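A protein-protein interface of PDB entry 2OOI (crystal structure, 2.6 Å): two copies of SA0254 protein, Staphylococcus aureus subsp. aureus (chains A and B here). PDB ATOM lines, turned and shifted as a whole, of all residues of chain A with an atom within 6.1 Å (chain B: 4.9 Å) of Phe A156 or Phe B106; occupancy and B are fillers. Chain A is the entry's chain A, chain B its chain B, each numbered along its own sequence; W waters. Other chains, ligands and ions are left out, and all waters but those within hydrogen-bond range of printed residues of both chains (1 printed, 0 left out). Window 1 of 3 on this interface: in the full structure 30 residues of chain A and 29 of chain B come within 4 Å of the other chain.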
ATOM      1  N   ARG A   2      30.700 -32.990   9.182  1.00  0.00           N
ATOM      2  CA  ARG A   2      30.365 -31.563   9.188  1.00  0.00           C
ATOM      3  C   ARG A   2      30.063 -30.963   7.822  1.00  0.00           C
ATOM      4  O   ARG A   2      30.754 -31.213   6.865  1.00  0.00           O
ATOM      5  CB  ARG A   2      31.534 -30.814   9.821  1.00  0.00           C
ATOM      6  CG  ARG A   2      31.149 -29.678  10.709  1.00  0.00           C
ATOM      7  CD  ARG A   2      31.870 -29.700  12.074  1.00  0.00           C
ATOM      8  NE  ARG A   2      31.293 -28.684  12.957  1.00  0.00           N
ATOM      9  CZ  ARG A   2      31.396 -28.662  14.278  1.00  0.00           C
ATOM     10  NH1 ARG A   2      32.065 -29.605  14.920  1.00  0.00           N
ATOM     11  NH2 ARG A   2      30.811 -27.680  14.957  1.00  0.00           N
ATOM     12  N   ILE A   3      29.026 -30.142   7.745  1.00  0.00           N
ATOM     13  CA  ILE A   3      28.614 -29.528   6.486  1.00  0.00           C
ATOM     14  C   ILE A   3      29.471 -28.303   6.178  1.00  0.00           C
ATOM     15  O   ILE A   3      29.636 -27.434   7.018  1.00  0.00           O
ATOM     16  CB  ILE A   3      27.125 -29.093   6.539  1.00  0.00           C
ATOM     17  CG1 ILE A   3      26.225 -30.298   6.826  1.00  0.00           C
ATOM     18  CG2 ILE A   3      26.720 -28.391   5.248  1.00  0.00           C
ATOM     19  CD1 ILE A   3      24.847 -29.922   7.269  1.00  0.00           C
ATOM     20  N   ASN A   4      29.992 -28.221   4.962  1.00  0.00           N
ATOM     21  CA  ASN A   4      30.795 -27.067   4.560  1.00  0.00           C
ATOM     22  C   ASN A   4      30.012 -26.069   3.698  1.00  0.00           C
ATOM     23  O   ASN A   4      29.519 -26.431   2.649  1.00  0.00           O
ATOM     24  CB  ASN A   4      32.047 -27.546   3.815  1.00  0.00           C
ATOM     25  CG  ASN A   4      33.063 -26.428   3.591  1.00  0.00           C
ATOM     26  OD1 ASN A   4      33.084 -25.443   4.328  1.00  0.00           O
ATOM     27  ND2 ASN A   4      33.912 -26.577   2.576  1.00  0.00           N
ATOM     28  N   VAL A   5      29.940 -24.809   4.123  1.00  0.00           N
ATOM     29  CA  VAL A   5      29.083 -23.815   3.456  1.00  0.00           C
ATOM     30  C   VAL A   5      29.752 -23.003   2.344  1.00  0.00           C
ATOM     31  O   VAL A   5      29.066 -22.513   1.464  1.00  0.00           O
ATOM     32  CB  VAL A   5      28.514 -22.753   4.465  1.00  0.00           C
ATOM     33  CG1 VAL A   5      27.210 -22.197   3.944  1.00  0.00           C
ATOM     34  CG2 VAL A   5      28.309 -23.335   5.869  1.00  0.00           C
ATOM     35  N   PHE A 106      21.801 -16.554   6.605  1.00  0.00           N
ATOM     36  CA  PHE A 106      21.168 -17.360   7.656  1.00  0.00           C
ATOM     37  C   PHE A 106      21.015 -16.725   9.063  1.00  0.00           C
ATOM     38  O   PHE A 106      21.723 -15.794   9.461  1.00  0.00           O
ATOM     39  CB  PHE A 106      21.855 -18.706   7.758  1.00  0.00           C
ATOM     40  CG  PHE A 106      23.292 -18.624   8.156  1.00  0.00           C
ATOM     41  CD1 PHE A 106      23.662 -18.715   9.504  1.00  0.00           C
ATOM     42  CD2 PHE A 106      24.281 -18.499   7.192  1.00  0.00           C
ATOM     43  CE1 PHE A 106      25.011 -18.667   9.886  1.00  0.00           C
ATOM     44  CE2 PHE A 106      25.635 -18.458   7.557  1.00  0.00           C
ATOM     45  CZ  PHE A 106      25.999 -18.546   8.910  1.00  0.00           C
ATOM     46  N   LEU A 128      18.048 -23.578  12.252  1.00  0.00           N
ATOM     47  CA  LEU A 128      18.749 -22.623  11.422  1.00  0.00           C
ATOM     48  C   LEU A 128      17.910 -22.373  10.173  1.00  0.00           C
ATOM     49  O   LEU A 128      17.521 -23.329   9.493  1.00  0.00           O
ATOM     50  CB  LEU A 128      20.107 -23.170  11.001  1.00  0.00           C
ATOM     51  CG  LEU A 128      21.004 -22.062  10.425  1.00  0.00           C
ATOM     52  CD1 LEU A 128      21.481 -21.095  11.580  1.00  0.00           C
ATOM     53  CD2 LEU A 128      22.175 -22.615   9.626  1.00  0.00           C
ATOM     54  N   TYR A 130      18.179 -20.927   6.486  1.00  0.00           N
ATOM     55  CA  TYR A 130      19.272 -20.716   5.563  1.00  0.00           C
ATOM     56  C   TYR A 130      18.694 -20.483   4.154  1.00  0.00           C
ATOM     57  O   TYR A 130      17.866 -21.240   3.653  1.00  0.00           O
ATOM     58  CB  TYR A 130      20.169 -21.925   5.689  1.00  0.00           C
ATOM     59  CG  TYR A 130      21.302 -22.077   4.723  1.00  0.00           C
ATOM     60  CD1 TYR A 130      22.628 -22.010   5.143  1.00  0.00           C
ATOM     61  CD2 TYR A 130      21.049 -22.377   3.401  1.00  0.00           C
ATOM     62  CE1 TYR A 130      23.670 -22.200   4.240  1.00  0.00           C
ATOM     63  CE2 TYR A 130      22.067 -22.572   2.512  1.00  0.00           C
ATOM     64  CZ  TYR A 130      23.362 -22.487   2.924  1.00  0.00           C
ATOM     65  OH  TYR A 130      24.311 -22.707   1.964  1.00  0.00           O
ATOM     66  N   PHE A 149      17.178 -26.229   9.010  1.00  0.00           N
ATOM     67  CA  PHE A 149      17.991 -27.333   9.500  1.00  0.00           C
ATOM     68  C   PHE A 149      17.546 -27.845  10.847  1.00  0.00           C
ATOM     69  O   PHE A 149      17.022 -27.102  11.673  1.00  0.00           O
ATOM     70  CB  PHE A 149      19.436 -26.917   9.611  1.00  0.00           C
ATOM     71  CG  PHE A 149      20.144 -26.796   8.299  1.00  0.00           C
ATOM     72  CD1 PHE A 149      20.278 -25.562   7.678  1.00  0.00           C
ATOM     73  CD2 PHE A 149      20.694 -27.907   7.699  1.00  0.00           C
ATOM     74  CE1 PHE A 149      20.951 -25.436   6.464  1.00  0.00           C
ATOM     75  CE2 PHE A 149      21.375 -27.800   6.476  1.00  0.00           C
ATOM     76  CZ  PHE A 149      21.507 -26.562   5.861  1.00  0.00           C
ATOM     77  N   ALA A 154      22.657 -30.843  12.316  1.00  0.00           N
ATOM     78  CA  ALA A 154      23.360 -29.945  11.401  1.00  0.00           C
ATOM     79  C   ALA A 154      24.517 -29.259  12.127  1.00  0.00           C
ATOM     80  O   ALA A 154      24.310 -28.495  13.072  1.00  0.00           O
ATOM     81  CB  ALA A 154      22.392 -28.909  10.803  1.00  0.00           C
ATOM     82  N   GLN A 155      25.728 -29.551  11.664  1.00  0.00           N
ATOM     83  CA  GLN A 155      26.987 -29.057  12.228  1.00  0.00           C
ATOM     84  C   GLN A 155      27.738 -28.459  11.068  1.00  0.00           C
ATOM     85  O   GLN A 155      27.787 -29.065  10.041  1.00  0.00           O
ATOM     86  CB  GLN A 155      27.777 -30.219  12.781  1.00  0.00           C
ATOM     87  CG  GLN A 155      26.957 -31.166  13.661  1.00  0.00           C
ATOM     88  CD  GLN A 155      26.569 -30.511  14.979  1.00  0.00           C
ATOM     89  OE1 GLN A 155      27.426 -29.915  15.671  1.00  0.00           O
ATOM     90  NE2 GLN A 155      25.277 -30.614  15.345  1.00  0.00           N
ATOM     91  N   PHE A 156      28.290 -27.267  11.203  1.00  0.00           N
ATOM     92  CA  PHE A 156      28.822 -26.544  10.052  1.00  0.00           C
ATOM     93  C   PHE A 156      30.278 -26.188  10.225  1.00  0.00           C
ATOM     94  O   PHE A 156      30.788 -26.106  11.351  1.00  0.00           O
ATOM     95  CB  PHE A 156      28.026 -25.260   9.801  1.00  0.00           C
ATOM     96  CG  PHE A 156      26.562 -25.501   9.537  1.00  0.00           C
ATOM     97  CD1 PHE A 156      25.662 -25.673  10.588  1.00  0.00           C
ATOM     98  CD2 PHE A 156      26.076 -25.568   8.236  1.00  0.00           C
ATOM     99  CE1 PHE A 156      24.302 -25.893  10.332  1.00  0.00           C
ATOM    100  CE2 PHE A 156      24.738 -25.784   7.990  1.00  0.00           C
ATOM    101  CZ  PHE A 156      23.850 -25.951   9.031  1.00  0.00           C
ATOM    102  N   TYR A 157      30.937 -25.964   9.095  1.00  0.00           N
ATOM    103  CA  TYR A 157      32.341 -25.648   9.070  1.00  0.00           C
ATOM    104  C   TYR A 157      32.646 -24.706   7.942  1.00  0.00           C
ATOM    105  O   TYR A 157      32.055 -24.793   6.884  1.00  0.00           O
ATOM    106  CB  TYR A 157      33.178 -26.914   8.884  1.00  0.00           C
ATOM    107  CG  TYR A 157      34.611 -26.595   8.525  1.00  0.00           C
ATOM    108  CD1 TYR A 157      35.462 -26.016   9.465  1.00  0.00           C
ATOM    109  CD2 TYR A 157      35.110 -26.831   7.239  1.00  0.00           C
ATOM    110  CE1 TYR A 157      36.786 -25.690   9.152  1.00  0.00           C
ATOM    111  CE2 TYR A 157      36.424 -26.514   6.905  1.00  0.00           C
ATOM    112  CZ  TYR A 157      37.267 -25.942   7.874  1.00  0.00           C
ATOM    113  OH  TYR A 157      38.577 -25.616   7.583  1.00  0.00           O
ATOM    114  N   ILE A 158      33.587 -23.800   8.147  1.00  0.00           N
ATOM    115  CA  ILE A 158      34.117 -23.064   7.013  1.00  0.00           C
ATOM    116  C   ILE A 158      35.585 -22.696   7.253  1.00  0.00           C
ATOM    117  O   ILE A 158      35.979 -22.479   8.384  1.00  0.00           O
ATOM    118  CB  ILE A 158      33.177 -21.905   6.605  1.00  0.00           C
ATOM    119  CG1 ILE A 158      31.830 -22.389   6.124  1.00  0.00           C
ATOM    120  CG2 ILE A 158      33.780 -21.013   5.525  1.00  0.00           C
ATOM    121  CD1 ILE A 158      30.887 -21.221   5.976  1.00  0.00           C
ATOM    122  N   ILE B 104      36.465 -22.096  11.087  1.00  0.00           N
ATOM    123  CA  ILE B 104      35.226 -21.712  11.737  1.00  0.00           C
ATOM    124  C   ILE B 104      34.310 -22.921  11.851  1.00  0.00           C
ATOM    125  O   ILE B 104      34.128 -23.665  10.894  1.00  0.00           O
ATOM    126  CB  ILE B 104      34.533 -20.654  10.929  1.00  0.00           C
ATOM    127  CG1 ILE B 104      35.297 -19.335  11.022  1.00  0.00           C
ATOM    128  CG2 ILE B 104      33.105 -20.493  11.400  1.00  0.00           C
ATOM    129  CD1 ILE B 104      34.990 -18.366   9.884  1.00  0.00           C
ATOM    130  N   PHE B 105      33.726 -23.107  13.023  1.00  0.00           N
ATOM    131  CA  PHE B 105      32.780 -24.186  13.242  1.00  0.00           C
ATOM    132  C   PHE B 105      31.524 -23.577  13.827  1.00  0.00           C
ATOM    133  O   PHE B 105      31.619 -22.776  14.744  1.00  0.00           O
ATOM    134  CB  PHE B 105      33.361 -25.224  14.207  1.00  0.00           C
ATOM    135  CG  PHE B 105      34.668 -25.812  13.744  1.00  0.00           C
ATOM    136  CD1 PHE B 105      34.697 -27.000  13.017  1.00  0.00           C
ATOM    137  CD2 PHE B 105      35.863 -25.164  13.990  1.00  0.00           C
ATOM    138  CE1 PHE B 105      35.917 -27.544  12.562  1.00  0.00           C
ATOM    139  CE2 PHE B 105      37.063 -25.704  13.549  1.00  0.00           C
ATOM    140  CZ  PHE B 105      37.087 -26.899  12.829  1.00  0.00           C
ATOM    141  N   PHE B 106      30.337 -23.911  13.310  1.00  0.00           N
ATOM    142  CA  PHE B 106      29.140 -23.462  14.018  1.00  0.00           C
ATOM    143  C   PHE B 106      27.974 -24.430  14.037  1.00  0.00           C
ATOM    144  O   PHE B 106      27.763 -25.202  13.107  1.00  0.00           O
ATOM    145  CB  PHE B 106      28.737 -22.070  13.564  1.00  0.00           C
ATOM    146  CG  PHE B 106      28.284 -21.981  12.126  1.00  0.00           C
ATOM    147  CD1 PHE B 106      26.951 -22.251  11.778  1.00  0.00           C
ATOM    148  CD2 PHE B 106      29.154 -21.517  11.136  1.00  0.00           C
ATOM    149  CE1 PHE B 106      26.513 -22.127  10.468  1.00  0.00           C
ATOM    150  CE2 PHE B 106      28.735 -21.403   9.816  1.00  0.00           C
ATOM    151  CZ  PHE B 106      27.396 -21.696   9.481  1.00  0.00           C
ATOM    152  N   ASN B 107      27.232 -24.417  15.135  1.00  0.00           N
ATOM    153  CA  ASN B 107      25.982 -25.155  15.188  1.00  0.00           C
ATOM    154  C   ASN B 107      24.947 -24.420  16.009  1.00  0.00           C
ATOM    155  O   ASN B 107      25.258 -23.441  16.661  1.00  0.00           O
ATOM    156  CB  ASN B 107      26.212 -26.549  15.723  1.00  0.00           C
ATOM    157  CG  ASN B 107      26.785 -26.539  17.101  1.00  0.00           C
ATOM    158  OD1 ASN B 107      26.203 -25.955  18.053  1.00  0.00           O
ATOM    159  ND2 ASN B 107      27.932 -27.170  17.238  1.00  0.00           N
ATOM    160  N   VAL B 108      23.704 -24.866  15.945  1.00  0.00           N
ATOM    161  CA  VAL B 108      22.610 -24.183  16.633  1.00  0.00           C
ATOM    162  C   VAL B 108      22.340 -25.006  17.869  1.00  0.00           C
ATOM    163  O   VAL B 108      22.458 -26.219  17.814  1.00  0.00           O
ATOM    164  CB  VAL B 108      21.363 -24.081  15.710  1.00  0.00           C
ATOM    165  CG1 VAL B 108      20.117 -23.610  16.470  1.00  0.00           C
ATOM    166  CG2 VAL B 108      21.689 -23.180  14.568  1.00  0.00           C
ATOM    167  N   LEU B 128      23.309 -19.395  18.373  1.00  0.00           N
ATOM    168  CA  LEU B 128      24.361 -19.958  17.529  1.00  0.00           C
ATOM    169  C   LEU B 128      25.604 -20.073  18.382  1.00  0.00           C
ATOM    170  O   LEU B 128      26.036 -19.081  18.980  1.00  0.00           O
ATOM    171  CB  LEU B 128      24.667 -19.043  16.327  1.00  0.00           C
ATOM    172  CG  LEU B 128      25.476 -19.661  15.169  1.00  0.00           C
ATOM    173  CD1 LEU B 128      24.661 -20.754  14.504  1.00  0.00           C
ATOM    174  CD2 LEU B 128      25.894 -18.640  14.121  1.00  0.00           C
ATOM    175  N   ARG B 129      26.167 -21.271  18.461  1.00  0.00           N
ATOM    176  CA  ARG B 129      27.474 -21.496  19.100  1.00  0.00           C
ATOM    177  C   ARG B 129      28.484 -21.573  17.957  1.00  0.00           C
ATOM    178  O   ARG B 129      28.392 -22.443  17.091  1.00  0.00           O
ATOM    179  CB  ARG B 129      27.522 -22.764  19.960  1.00  0.00           C
ATOM    180  CG  ARG B 129      26.209 -23.175  20.562  1.00  0.00           C
ATOM    181  CD  ARG B 129      26.319 -24.064  21.791  1.00  0.00           C
ATOM    182  NE  ARG B 129      26.552 -23.168  22.915  1.00  0.00           N
ATOM    183  CZ  ARG B 129      25.737 -22.932  23.947  1.00  0.00           C
ATOM    184  NH1 ARG B 129      24.592 -23.565  24.162  1.00  0.00           N
ATOM    185  NH2 ARG B 129      26.113 -22.038  24.809  1.00  0.00           N
ATOM    186  N   TYR B 130      29.428 -20.646  17.961  1.00  0.00           N
ATOM    187  CA  TYR B 130      30.349 -20.411  16.865  1.00  0.00           C
ATOM    188  C   TYR B 130      31.759 -20.485  17.444  1.00  0.00           C
ATOM    189  O   TYR B 130      32.009 -19.968  18.524  1.00  0.00           O
ATOM    190  CB  TYR B 130      30.019 -19.027  16.348  1.00  0.00           C
ATOM    191  CG  TYR B 130      30.847 -18.407  15.256  1.00  0.00           C
ATOM    192  CD1 TYR B 130      30.346 -18.287  13.955  1.00  0.00           C
ATOM    193  CD2 TYR B 130      32.088 -17.828  15.543  1.00  0.00           C
ATOM    194  CE1 TYR B 130      31.076 -17.647  12.957  1.00  0.00           C
ATOM    195  CE2 TYR B 130      32.828 -17.173  14.551  1.00  0.00           C
ATOM    196  CZ  TYR B 130      32.315 -17.090  13.269  1.00  0.00           C
ATOM    197  OH  TYR B 130      33.057 -16.435  12.299  1.00  0.00           O
HETATM  198  O   HOH W   1      30.661 -25.167  17.311  1.00  0.00           O
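Of the printed residues of chain B, Ala A154 touches Asn B107 (3.8 Å).
Of chain B, only Phe B105 and Phe B106 come within 4 Å of Phe A156.
Of the printed residues of chain B, Ile A158 touches Ile B104.
Of the printed residues of chain A, Phe B105 touches Arg A2 (3.6 Å), Phe A156 (3.4 Å) and Tyr A157 (3.5 Å).
Of chain A, only Phe A106 (3.5 Å), Gln A155 (3.8 Å) and Phe A156 (2.9 Å) come within 4 Å of Phe B106.
Of the printed residues of chain A, Asn B107 touches Arg A2, Ala A154 and Gln A155.
The nearest printed residue of chain B that does not touch Gln A155 is Val B108 (5.8 Å).
O of Gln A155 sits at hydrogen-bond distance from N of Ile A3.
O of Leu A128 is in hydrogen-bond range of N of Phe A149, 3.0 Å away.
The backbone carbonyl oxygen (O) of Tyr A157 lies close to the side-chain amide oxygen (OD1) of Asn A4, 2.8 Å away.
The backbone carbonyl oxygen (O) of Phe A156 is in hydrogen-bond range of the guanidinium group (NE) of Arg A2 (3.1 Å).
The backbone NH (N) of Tyr A157 sits at hydrogen-bond distance from the backbone carbonyl oxygen (O) of Ile A3 (2.9 Å).
The backbone NH (N) of Val A5 sits at hydrogen-bond distance from the backbone carbonyl oxygen (O) of Tyr A157.
Hydrophobic or aromatic side chains of chain B that line the printed part of chain A: Ile B104, Phe B105, Phe B106 and Val B108.
Of the 13 printed residues of chain A, 8 touch a printed residue of chain B.
Hydrophobic or aromatic side chains of chain A that line the printed part of chain B: Phe A106, Leu A128, Phe A156 and Tyr A157.
Along chain A the printed residues that touch a printed residue of chain B span positions 2 to 158.
Phe B106 touches its own counterpart, Phe A106.
Of the 12 pairs that touch across the chains among the printed residues, 1 has its exchanged pair printed and touching as well.
Water W1 bridges ND2 of Asn B107 (3.4 Å) and NH2 of Arg A2 (3.4 Å).
Among the printed residues, merely in contact across the chains: Arg A2 with Phe B105 (3.6 Å), Arg A2 with Asn B107 (3.7 Å), Phe A106 with Phe B106 (3.5 Å), Leu A128 with Val B108 (3.6 Å), Ala A154 with Asn B107 (3.8 Å), Gln A155 with Phe B106 (3.8 Å), Phe A156 with Phe B105 (3.4 Å), Tyr A157 with Ile B104 (3.1 Å) and Tyr A157 with Phe B105 (3.5 Å).
The backbone carbonyl oxygen (O) of Phe B106 lies within hydrogen-bond range of the backbone NH (N) of Phe A156 (2.9 Å).
OE1 of Gln A155 is in hydrogen-bond range of ND2 of Asn B107, 3.2 Å away.
The backbone NH of Ile B104 sits at hydrogen-bond distance from the backbone carbonyl oxygen of Ile A158, 2.8 Å away.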
